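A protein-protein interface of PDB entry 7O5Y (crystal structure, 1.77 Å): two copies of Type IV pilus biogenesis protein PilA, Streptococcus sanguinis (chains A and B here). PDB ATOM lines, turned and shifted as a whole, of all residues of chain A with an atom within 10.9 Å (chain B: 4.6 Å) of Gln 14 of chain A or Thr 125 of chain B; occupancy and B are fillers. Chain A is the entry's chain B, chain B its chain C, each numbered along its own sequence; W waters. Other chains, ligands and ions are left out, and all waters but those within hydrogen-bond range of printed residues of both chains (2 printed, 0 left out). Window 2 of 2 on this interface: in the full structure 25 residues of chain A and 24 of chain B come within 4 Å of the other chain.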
ATOM      1  N   GLN A  12      31.960  11.373   3.556  1.00  0.00           N
ATOM      2  CA  GLN A  12      32.298  10.686   4.800  1.00  0.00           C
ATOM      3  C   GLN A  12      31.533   9.374   4.953  1.00  0.00           C
ATOM      4  O   GLN A  12      32.122   8.298   4.893  1.00  0.00           O
ATOM      5  CB  GLN A  12      32.029  11.589   6.003  1.00  0.00           C
ATOM      6  CG  GLN A  12      33.297  12.075   6.681  1.00  0.00           C
ATOM      7  CD  GLN A  12      34.242  10.937   7.039  1.00  0.00           C
ATOM      8  OE1 GLN A  12      33.814   9.805   7.281  1.00  0.00           O
ATOM      9  NE2 GLN A  12      35.537  11.237   7.073  1.00  0.00           N
ATOM     10  N   SER A  13      30.223   9.471   5.174  1.00  0.00           N
ATOM     11  CA  SER A  13      29.367   8.297   5.110  1.00  0.00           C
ATOM     12  C   SER A  13      29.310   7.770   3.678  1.00  0.00           C
ATOM     13  O   SER A  13      29.630   8.473   2.717  1.00  0.00           O
ATOM     14  CB  SER A  13      27.954   8.632   5.595  1.00  0.00           C
ATOM     15  OG  SER A  13      27.312   9.553   4.731  1.00  0.00           O
ATOM     16  N   GLN A  14      28.892   6.510   3.538  1.00  0.00           N
ATOM     17  CA  GLN A  14      28.651   5.985   2.200  1.00  0.00           C
ATOM     18  C   GLN A  14      27.457   6.667   1.549  1.00  0.00           C
ATOM     19  O   GLN A  14      27.411   6.806   0.320  1.00  0.00           O
ATOM     20  CB  GLN A  14      28.447   4.469   2.251  1.00  0.00           C
ATOM     21  CG  GLN A  14      29.696   3.719   2.654  1.00  0.00           C
ATOM     22  CD  GLN A  14      30.811   3.935   1.659  1.00  0.00           C
ATOM     23  OE1 GLN A  14      30.702   3.533   0.506  1.00  0.00           O
ATOM     24  NE2 GLN A  14      31.878   4.598   2.092  1.00  0.00           N
ATOM     25  N   THR A  15      26.483   7.096   2.351  1.00  0.00           N
ATOM     26  CA  THR A  15      25.388   7.895   1.816  1.00  0.00           C
ATOM     27  C   THR A  15      25.917   9.187   1.203  1.00  0.00           C
ATOM     28  O   THR A  15      25.551   9.557   0.077  1.00  0.00           O
ATOM     29  CB  THR A  15      24.375   8.193   2.925  1.00  0.00           C
ATOM     30  OG1 THR A  15      23.662   6.991   3.252  1.00  0.00           O
ATOM     31  CG2 THR A  15      23.387   9.256   2.475  1.00  0.00           C
ATOM     32  N   GLN A  16      26.804   9.874   1.924  1.00  0.00           N
ATOM     33  CA  GLN A  16      27.364  11.115   1.405  1.00  0.00           C
ATOM     34  C   GLN A  16      28.284  10.844   0.224  1.00  0.00           C
ATOM     35  O   GLN A  16      28.293  11.609  -0.747  1.00  0.00           O
ATOM     36  CB  GLN A  16      28.102  11.871   2.512  1.00  0.00           C
ATOM     37  CG  GLN A  16      28.466  13.308   2.136  1.00  0.00           C
ATOM     38  CD  GLN A  16      27.257  14.125   1.707  1.00  0.00           C
ATOM     39  OE1 GLN A  16      26.276  14.235   2.441  1.00  0.00           O
ATOM     40  NE2 GLN A  16      27.319  14.690   0.505  1.00  0.00           N
ATOM     41  N   ARG A  17      29.043   9.745   0.274  1.00  0.00           N
ATOM     42  CA  ARG A  17      29.896   9.394  -0.859  1.00  0.00           C
ATOM     43  C   ARG A  17      29.091   9.264  -2.153  1.00  0.00           C
ATOM     44  O   ARG A  17      29.532   9.726  -3.210  1.00  0.00           O
ATOM     45  CB  ARG A  17      30.664   8.107  -0.560  1.00  0.00           C
ATOM     46  CG  ARG A  17      31.405   7.551  -1.765  1.00  0.00           C
ATOM     47  CD  ARG A  17      32.618   8.404  -2.159  1.00  0.00           C
ATOM     48  NE  ARG A  17      33.505   7.650  -3.046  1.00  0.00           N
ATOM     49  CZ  ARG A  17      34.739   8.008  -3.392  1.00  0.00           C
ATOM     50  NH1 ARG A  17      35.271   9.139  -2.935  1.00  0.00           N
ATOM     51  NH2 ARG A  17      35.445   7.226  -4.198  1.00  0.00           N
ATOM     52  N   MET A  18      27.911   8.652  -2.093  1.00  0.00           N
ATOM     53  CA  MET A  18      27.049   8.565  -3.271  1.00  0.00           C
ATOM     54  C   MET A  18      26.680   9.933  -3.813  1.00  0.00           C
ATOM     55  O   MET A  18      26.760  10.192  -5.018  1.00  0.00           O
ATOM     56  CB  MET A  18      25.767   7.799  -2.937  1.00  0.00           C
ATOM     57  CG  MET A  18      24.762   7.538  -4.093  1.00  0.00           C
ATOM     58  SD  MET A  18      25.403   6.561  -5.614  1.00  0.00           S
ATOM     59  CE  MET A  18      24.598   7.321  -7.145  1.00  0.00           C
ATOM     60  N   TYR A  19      26.203  10.789  -2.915  1.00  0.00           N
ATOM     61  CA  TYR A  19      25.838  12.134  -3.333  1.00  0.00           C
ATOM     62  C   TYR A  19      27.046  12.864  -3.907  1.00  0.00           C
ATOM     63  O   TYR A  19      26.922  13.611  -4.886  1.00  0.00           O
ATOM     64  CB  TYR A  19      25.240  12.905  -2.159  1.00  0.00           C
ATOM     65  CG  TYR A  19      23.793  12.572  -1.848  1.00  0.00           C
ATOM     66  CD1 TYR A  19      22.785  12.822  -2.768  1.00  0.00           C
ATOM     67  CD2 TYR A  19      23.440  12.033  -0.620  1.00  0.00           C
ATOM     68  CE1 TYR A  19      21.465  12.529  -2.479  1.00  0.00           C
ATOM     69  CE2 TYR A  19      22.124  11.748  -0.318  1.00  0.00           C
ATOM     70  CZ  TYR A  19      21.144  11.992  -1.248  1.00  0.00           C
ATOM     71  OH  TYR A  19      19.834  11.698  -0.952  1.00  0.00           O
ATOM     72  N   ASN A  20      28.233  12.631  -3.332  1.00  0.00           N
ATOM     73  CA  ASN A  20      29.439  13.283  -3.837  1.00  0.00           C
ATOM     74  C   ASN A  20      29.803  12.780  -5.229  1.00  0.00           C
ATOM     75  O   ASN A  20      30.188  13.572  -6.096  1.00  0.00           O
ATOM     76  CB  ASN A  20      30.602  13.073  -2.864  1.00  0.00           C
ATOM     77  CG  ASN A  20      30.402  13.821  -1.554  1.00  0.00           C
ATOM     78  OD1 ASN A  20      29.553  14.703  -1.460  1.00  0.00           O
ATOM     79  ND2 ASN A  20      31.187  13.470  -0.542  1.00  0.00           N
ATOM     80  N   TYR A  21      29.694  11.467  -5.458  1.00  0.00           N
ATOM     81  CA  TYR A  21      29.897  10.909  -6.793  1.00  0.00           C
ATOM     82  C   TYR A  21      28.957  11.542  -7.813  1.00  0.00           C
ATOM     83  O   TYR A  21      29.379  11.920  -8.913  1.00  0.00           O
ATOM     84  CB  TYR A  21      29.709   9.385  -6.757  1.00  0.00           C
ATOM     85  CG  TYR A  21      29.357   8.789  -8.099  1.00  0.00           C
ATOM     86  CD1 TYR A  21      30.302   8.725  -9.121  1.00  0.00           C
ATOM     87  CD2 TYR A  21      28.082   8.298  -8.353  1.00  0.00           C
ATOM     88  CE1 TYR A  21      29.985   8.193 -10.355  1.00  0.00           C
ATOM     89  CE2 TYR A  21      27.757   7.756  -9.587  1.00  0.00           C
ATOM     90  CZ  TYR A  21      28.711   7.703 -10.581  1.00  0.00           C
ATOM     91  OH  TYR A  21      28.400   7.185 -11.816  1.00  0.00           O
ATOM     92  N   LEU A  22      27.668  11.660  -7.469  1.00  0.00           N
ATOM     93  CA  LEU A  22      26.699  12.246  -8.389  1.00  0.00           C
ATOM     94  C   LEU A  22      27.004  13.706  -8.678  1.00  0.00           C
ATOM     95  O   LEU A  22      26.874  14.161  -9.821  1.00  0.00           O
ATOM     96  CB  LEU A  22      25.291  12.122  -7.813  1.00  0.00           C
ATOM     97  CG  LEU A  22      24.849  10.669  -7.724  1.00  0.00           C
ATOM     98  CD1 LEU A  22      23.513  10.578  -7.019  1.00  0.00           C
ATOM     99  CD2 LEU A  22      24.759  10.054  -9.117  1.00  0.00           C
ATOM    100  N   LEU A 108      35.598  14.337  -6.283  1.00  0.00           N
ATOM    101  CA  LEU A 108      34.528  14.110  -5.321  1.00  0.00           C
ATOM    102  C   LEU A 108      34.863  14.814  -4.013  1.00  0.00           C
ATOM    103  O   LEU A 108      36.013  14.802  -3.571  1.00  0.00           O
ATOM    104  CB  LEU A 108      34.337  12.613  -5.069  1.00  0.00           C
ATOM    105  CG  LEU A 108      33.542  11.836  -6.117  1.00  0.00           C
ATOM    106  CD1 LEU A 108      34.284  11.736  -7.450  1.00  0.00           C
ATOM    107  CD2 LEU A 108      33.221  10.441  -5.575  1.00  0.00           C
ATOM    108  N   ALA A 109      33.855  15.423  -3.393  1.00  0.00           N
ATOM    109  CA  ALA A 109      34.105  16.184  -2.175  1.00  0.00           C
ATOM    110  C   ALA A 109      34.742  15.296  -1.112  1.00  0.00           C
ATOM    111  O   ALA A 109      34.392  14.122  -0.969  1.00  0.00           O
ATOM    112  CB  ALA A 109      32.806  16.805  -1.655  1.00  0.00           C
ATOM    113  N   GLY A 110      35.718  15.850  -0.396  1.00  0.00           N
ATOM    114  CA  GLY A 110      36.423  15.090   0.618  1.00  0.00           C
ATOM    115  C   GLY A 110      37.301  13.976   0.100  1.00  0.00           C
ATOM    116  O   GLY A 110      37.711  13.112   0.882  1.00  0.00           O
ATOM    117  N   SER A 111      37.615  13.969  -1.192  1.00  0.00           N
ATOM    118  CA  SER A 111      38.379  12.883  -1.782  1.00  0.00           C
ATOM    119  C   SER A 111      39.230  13.449  -2.906  1.00  0.00           C
ATOM    120  O   SER A 111      38.959  14.531  -3.433  1.00  0.00           O
ATOM    121  CB  SER A 111      37.447  11.771  -2.301  1.00  0.00           C
ATOM    122  OG  SER A 111      38.149  10.756  -2.997  1.00  0.00           O
ATOM    123  N   ASP A 113      39.691  11.122  -5.402  1.00  0.00           N
ATOM    124  CA  ASP A 113      39.027  10.452  -6.509  1.00  0.00           C
ATOM    125  C   ASP A 113      38.215  11.472  -7.307  1.00  0.00           C
ATOM    126  O   ASP A 113      37.788  12.503  -6.791  1.00  0.00           O
ATOM    127  CB  ASP A 113      38.106   9.337  -6.005  1.00  0.00           C
ATOM    128  CG  ASP A 113      38.825   8.329  -5.128  1.00  0.00           C
ATOM    129  OD1 ASP A 113      40.065   8.192  -5.238  1.00  0.00           O
ATOM    130  OD2 ASP A 113      38.142   7.684  -4.311  1.00  0.00           O
ATOM    131  N   LEU A 135      34.032   7.157 -12.821  1.00  0.00           N
ATOM    132  CA  LEU A 135      34.676   7.388 -11.538  1.00  0.00           C
ATOM    133  C   LEU A 135      36.102   6.844 -11.598  1.00  0.00           C
ATOM    134  O   LEU A 135      36.330   5.733 -12.087  1.00  0.00           O
ATOM    135  CB  LEU A 135      33.879   6.706 -10.424  1.00  0.00           C
ATOM    136  CG  LEU A 135      34.450   6.778  -9.012  1.00  0.00           C
ATOM    137  CD1 LEU A 135      34.589   8.240  -8.585  1.00  0.00           C
ATOM    138  CD2 LEU A 135      33.599   5.977  -8.014  1.00  0.00           C
ATOM    139  N   TRP B  36      18.053   7.744  -5.286  1.00  0.00           N
ATOM    140  CA  TRP B  36      18.808   7.517  -4.060  1.00  0.00           C
ATOM    141  C   TRP B  36      18.090   8.117  -2.859  1.00  0.00           C
ATOM    142  O   TRP B  36      17.898   7.449  -1.837  1.00  0.00           O
ATOM    143  CB  TRP B  36      20.210   8.118  -4.215  1.00  0.00           C
ATOM    144  CG  TRP B  36      21.205   7.845  -3.108  1.00  0.00           C
ATOM    145  CD1 TRP B  36      21.908   8.779  -2.391  1.00  0.00           C
ATOM    146  CD2 TRP B  36      21.651   6.564  -2.634  1.00  0.00           C
ATOM    147  NE1 TRP B  36      22.745   8.161  -1.494  1.00  0.00           N
ATOM    148  CE2 TRP B  36      22.605   6.802  -1.620  1.00  0.00           C
ATOM    149  CE3 TRP B  36      21.330   5.240  -2.963  1.00  0.00           C
ATOM    150  CZ2 TRP B  36      23.242   5.770  -0.932  1.00  0.00           C
ATOM    151  CZ3 TRP B  36      21.960   4.216  -2.279  1.00  0.00           C
ATOM    152  CH2 TRP B  36      22.908   4.487  -1.272  1.00  0.00           C
ATOM    153  N   ASN B 122      25.676  -1.753  -2.558  1.00  0.00           N
ATOM    154  CA  ASN B 122      25.444  -2.887  -1.674  1.00  0.00           C
ATOM    155  C   ASN B 122      24.394  -2.539  -0.629  1.00  0.00           C
ATOM    156  O   ASN B 122      24.412  -1.453  -0.046  1.00  0.00           O
ATOM    157  CB  ASN B 122      26.741  -3.311  -0.985  1.00  0.00           C
ATOM    158  CG  ASN B 122      26.553  -4.524  -0.099  1.00  0.00           C
ATOM    159  OD1 ASN B 122      26.510  -4.413   1.124  1.00  0.00           O
ATOM    160  ND2 ASN B 122      26.447  -5.690  -0.714  1.00  0.00           N
ATOM    161  N   PHE B 123      23.474  -3.476  -0.393  1.00  0.00           N
ATOM    162  CA  PHE B 123      22.384  -3.198   0.535  1.00  0.00           C
ATOM    163  C   PHE B 123      22.906  -2.928   1.941  1.00  0.00           C
ATOM    164  O   PHE B 123      22.424  -2.022   2.626  1.00  0.00           O
ATOM    165  CB  PHE B 123      21.389  -4.356   0.554  1.00  0.00           C
ATOM    166  CG  PHE B 123      20.339  -4.214   1.612  1.00  0.00           C
ATOM    167  CD1 PHE B 123      19.219  -3.430   1.390  1.00  0.00           C
ATOM    168  CD2 PHE B 123      20.491  -4.828   2.845  1.00  0.00           C
ATOM    169  CE1 PHE B 123      18.257  -3.282   2.373  1.00  0.00           C
ATOM    170  CE2 PHE B 123      19.537  -4.678   3.832  1.00  0.00           C
ATOM    171  CZ  PHE B 123      18.419  -3.906   3.595  1.00  0.00           C
ATOM    172  N   ASP B 124      23.907  -3.689   2.377  1.00  0.00           N
ATOM    173  CA  ASP B 124      24.371  -3.589   3.755  1.00  0.00           C
ATOM    174  C   ASP B 124      25.232  -2.349   3.974  1.00  0.00           C
ATOM    175  O   ASP B 124      24.998  -1.577   4.911  1.00  0.00           O
ATOM    176  CB  ASP B 124      25.144  -4.852   4.131  1.00  0.00           C
ATOM    177  CG  ASP B 124      25.566  -4.860   5.579  1.00  0.00           C
ATOM    178  OD1 ASP B 124      24.674  -4.933   6.452  1.00  0.00           O
ATOM    179  OD2 ASP B 124      26.782  -4.774   5.844  1.00  0.00           O
ATOM    180  N   THR B 125      26.228  -2.135   3.116  1.00  0.00           N
ATOM    181  CA  THR B 125      27.179  -1.047   3.311  1.00  0.00           C
ATOM    182  C   THR B 125      26.756   0.261   2.658  1.00  0.00           C
ATOM    183  O   THR B 125      27.319   1.309   2.995  1.00  0.00           O
ATOM    184  CB  THR B 125      28.540  -1.425   2.732  1.00  0.00           C
ATOM    185  OG1 THR B 125      28.427  -1.482   1.304  1.00  0.00           O
ATOM    186  CG2 THR B 125      29.001  -2.781   3.259  1.00  0.00           C
ATOM    187  N   LYS B 126      25.819   0.215   1.708  1.00  0.00           N
ATOM    188  CA  LYS B 126      25.470   1.346   0.845  1.00  0.00           C
ATOM    189  C   LYS B 126      26.650   1.817  -0.007  1.00  0.00           C
ATOM    190  O   LYS B 126      26.605   2.901  -0.598  1.00  0.00           O
ATOM    191  CB  LYS B 126      24.888   2.514   1.652  1.00  0.00           C
ATOM    192  CG  LYS B 126      23.519   2.205   2.245  1.00  0.00           C
ATOM    193  CD  LYS B 126      22.991   3.356   3.085  1.00  0.00           C
ATOM    194  CE  LYS B 126      21.600   3.045   3.641  1.00  0.00           C
ATOM    195  NZ  LYS B 126      21.589   1.975   4.676  1.00  0.00           N
ATOM    196  N   GLY B 127      27.702   1.007  -0.113  1.00  0.00           N
ATOM    197  CA  GLY B 127      28.849   1.389  -0.918  1.00  0.00           C
ATOM    198  C   GLY B 127      28.602   1.137  -2.398  1.00  0.00           C
ATOM    199  O   GLY B 127      27.923   0.188  -2.787  1.00  0.00           O
ATOM    200  N   ILE B 128      29.171   2.009  -3.232  1.00  0.00           N
ATOM    201  CA  ILE B 128      29.092   1.821  -4.674  1.00  0.00           C
ATOM    202  C   ILE B 128      29.934   0.620  -5.081  1.00  0.00           C
ATOM    203  O   ILE B 128      31.125   0.541  -4.762  1.00  0.00           O
ATOM    204  CB  ILE B 128      29.561   3.080  -5.416  1.00  0.00           C
ATOM    205  CG1 ILE B 128      28.698   4.280  -5.033  1.00  0.00           C
ATOM    206  CG2 ILE B 128      29.525   2.834  -6.921  1.00  0.00           C
ATOM    207  CD1 ILE B 128      29.365   5.618  -5.348  1.00  0.00           C
HETATM  208  O   HOH W   1      27.997   5.054  -1.648  1.00  0.00           O
HETATM  209  O   HOH W   2      30.596   4.121  -2.085  1.00  0.00           O
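The backbone NH (N) of Asn 122 of chain B lies within hydrogen-bond range of the backbone carbonyl oxygen (O) of Gly 127 of chain B.
The backbone NH (N) of Gly 127 of chain B sits at hydrogen-bond distance from the side-chain hydroxyl (OG1) of Thr 125 of chain B (3.0 Å).
The side-chain amide oxygen (OD1) of Asn 122 of chain B is in hydrogen-bond range of the backbone NH (N) of Thr 125 of chain B, at 3.0 Å.
Thr 125 of chain B touches Gln 14 of chain A (O to CG, 3.4 Å).
Lys 126 of chain B touches Gln 14 of chain A.
Gly 127 of chain B touches Gln 14 of chain A.
Thr 15 of chain A touches Trp 36 of chain B.
Thr 15 of chain A touches Lys 126 of chain B (OG1 to CD, 3.7 Å).
CG of Met 18 of chain A touches NE1 of Trp 36 of chain B, 3.3 Å away.
Trp 36 of chain B touches Tyr 19 of chain A (CD1 to CZ, 3.5 Å).
Printed residues of chain B within 4 Å of Gln 14 of chain A: Thr 125, Lys 126 and Gly 127.
Of the printed residues of chain B, Thr 15 of chain A touches Trp 36 (3.5 Å) and Lys 126 (3.7 Å).
Printed residues of chain B within 4 Å of Tyr 19 of chain A: Trp 36.
Printed residues of chain A within 4 Å of Trp 36 of chain B: Thr 15 (3.5 Å), Met 18 (3.3 Å) and Tyr 19 (3.5 Å).
No residue of chain A comes within 4 Å of Asn 122 of chain B.
No residue of chain A comes within 4 Å of Asp 124 of chain B.
Thr 125 of chain B touches one residue of chain A.
Lys 126 of chain B touches two residues of chain A.
Gly 127 of chain B touches just one residue of chain A: Gln 14.
The nearest residue of chain A that does not touch Thr 125 of chain B is Thr 15 of chain A (5.9 Å).
The nearest printed residue of chain A that does not touch Trp 36 of chain B is Gln 14 of chain A (4.5 Å).
Of the 17 printed residues of chain A, 4 touch a printed residue of chain B.
Of the 8 printed residues of chain B, 4 touch a printed residue of chain A.
Hydrophobic or aromatic side chains of chain B within 4 Å of the printed part of chain A: Trp 36.
Among the printed residues, 7 pairs touch across the chains.
Among the printed residues, no Asp or Glu carboxylate lies within 4 Å of a Lys or Arg side-chain nitrogen of the other chain.
No position is printed for both chains.
Of the 7 pairs that touch across the chains among the printed residues, none has its exchanged pair printed and touching as well.
Water W2 bridges the side-chain amide oxygen of Gln 14 of chain A (2.7 Å) and the backbone NH of Ile 128 of chain B (2.8 Å).
Water W1 lies within hydrogen-bond range of the backbone carbonyl oxygen (O) of Gln 14 of chain A and the backbone carbonyl oxygen (O) of Lys 126 of chain B.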
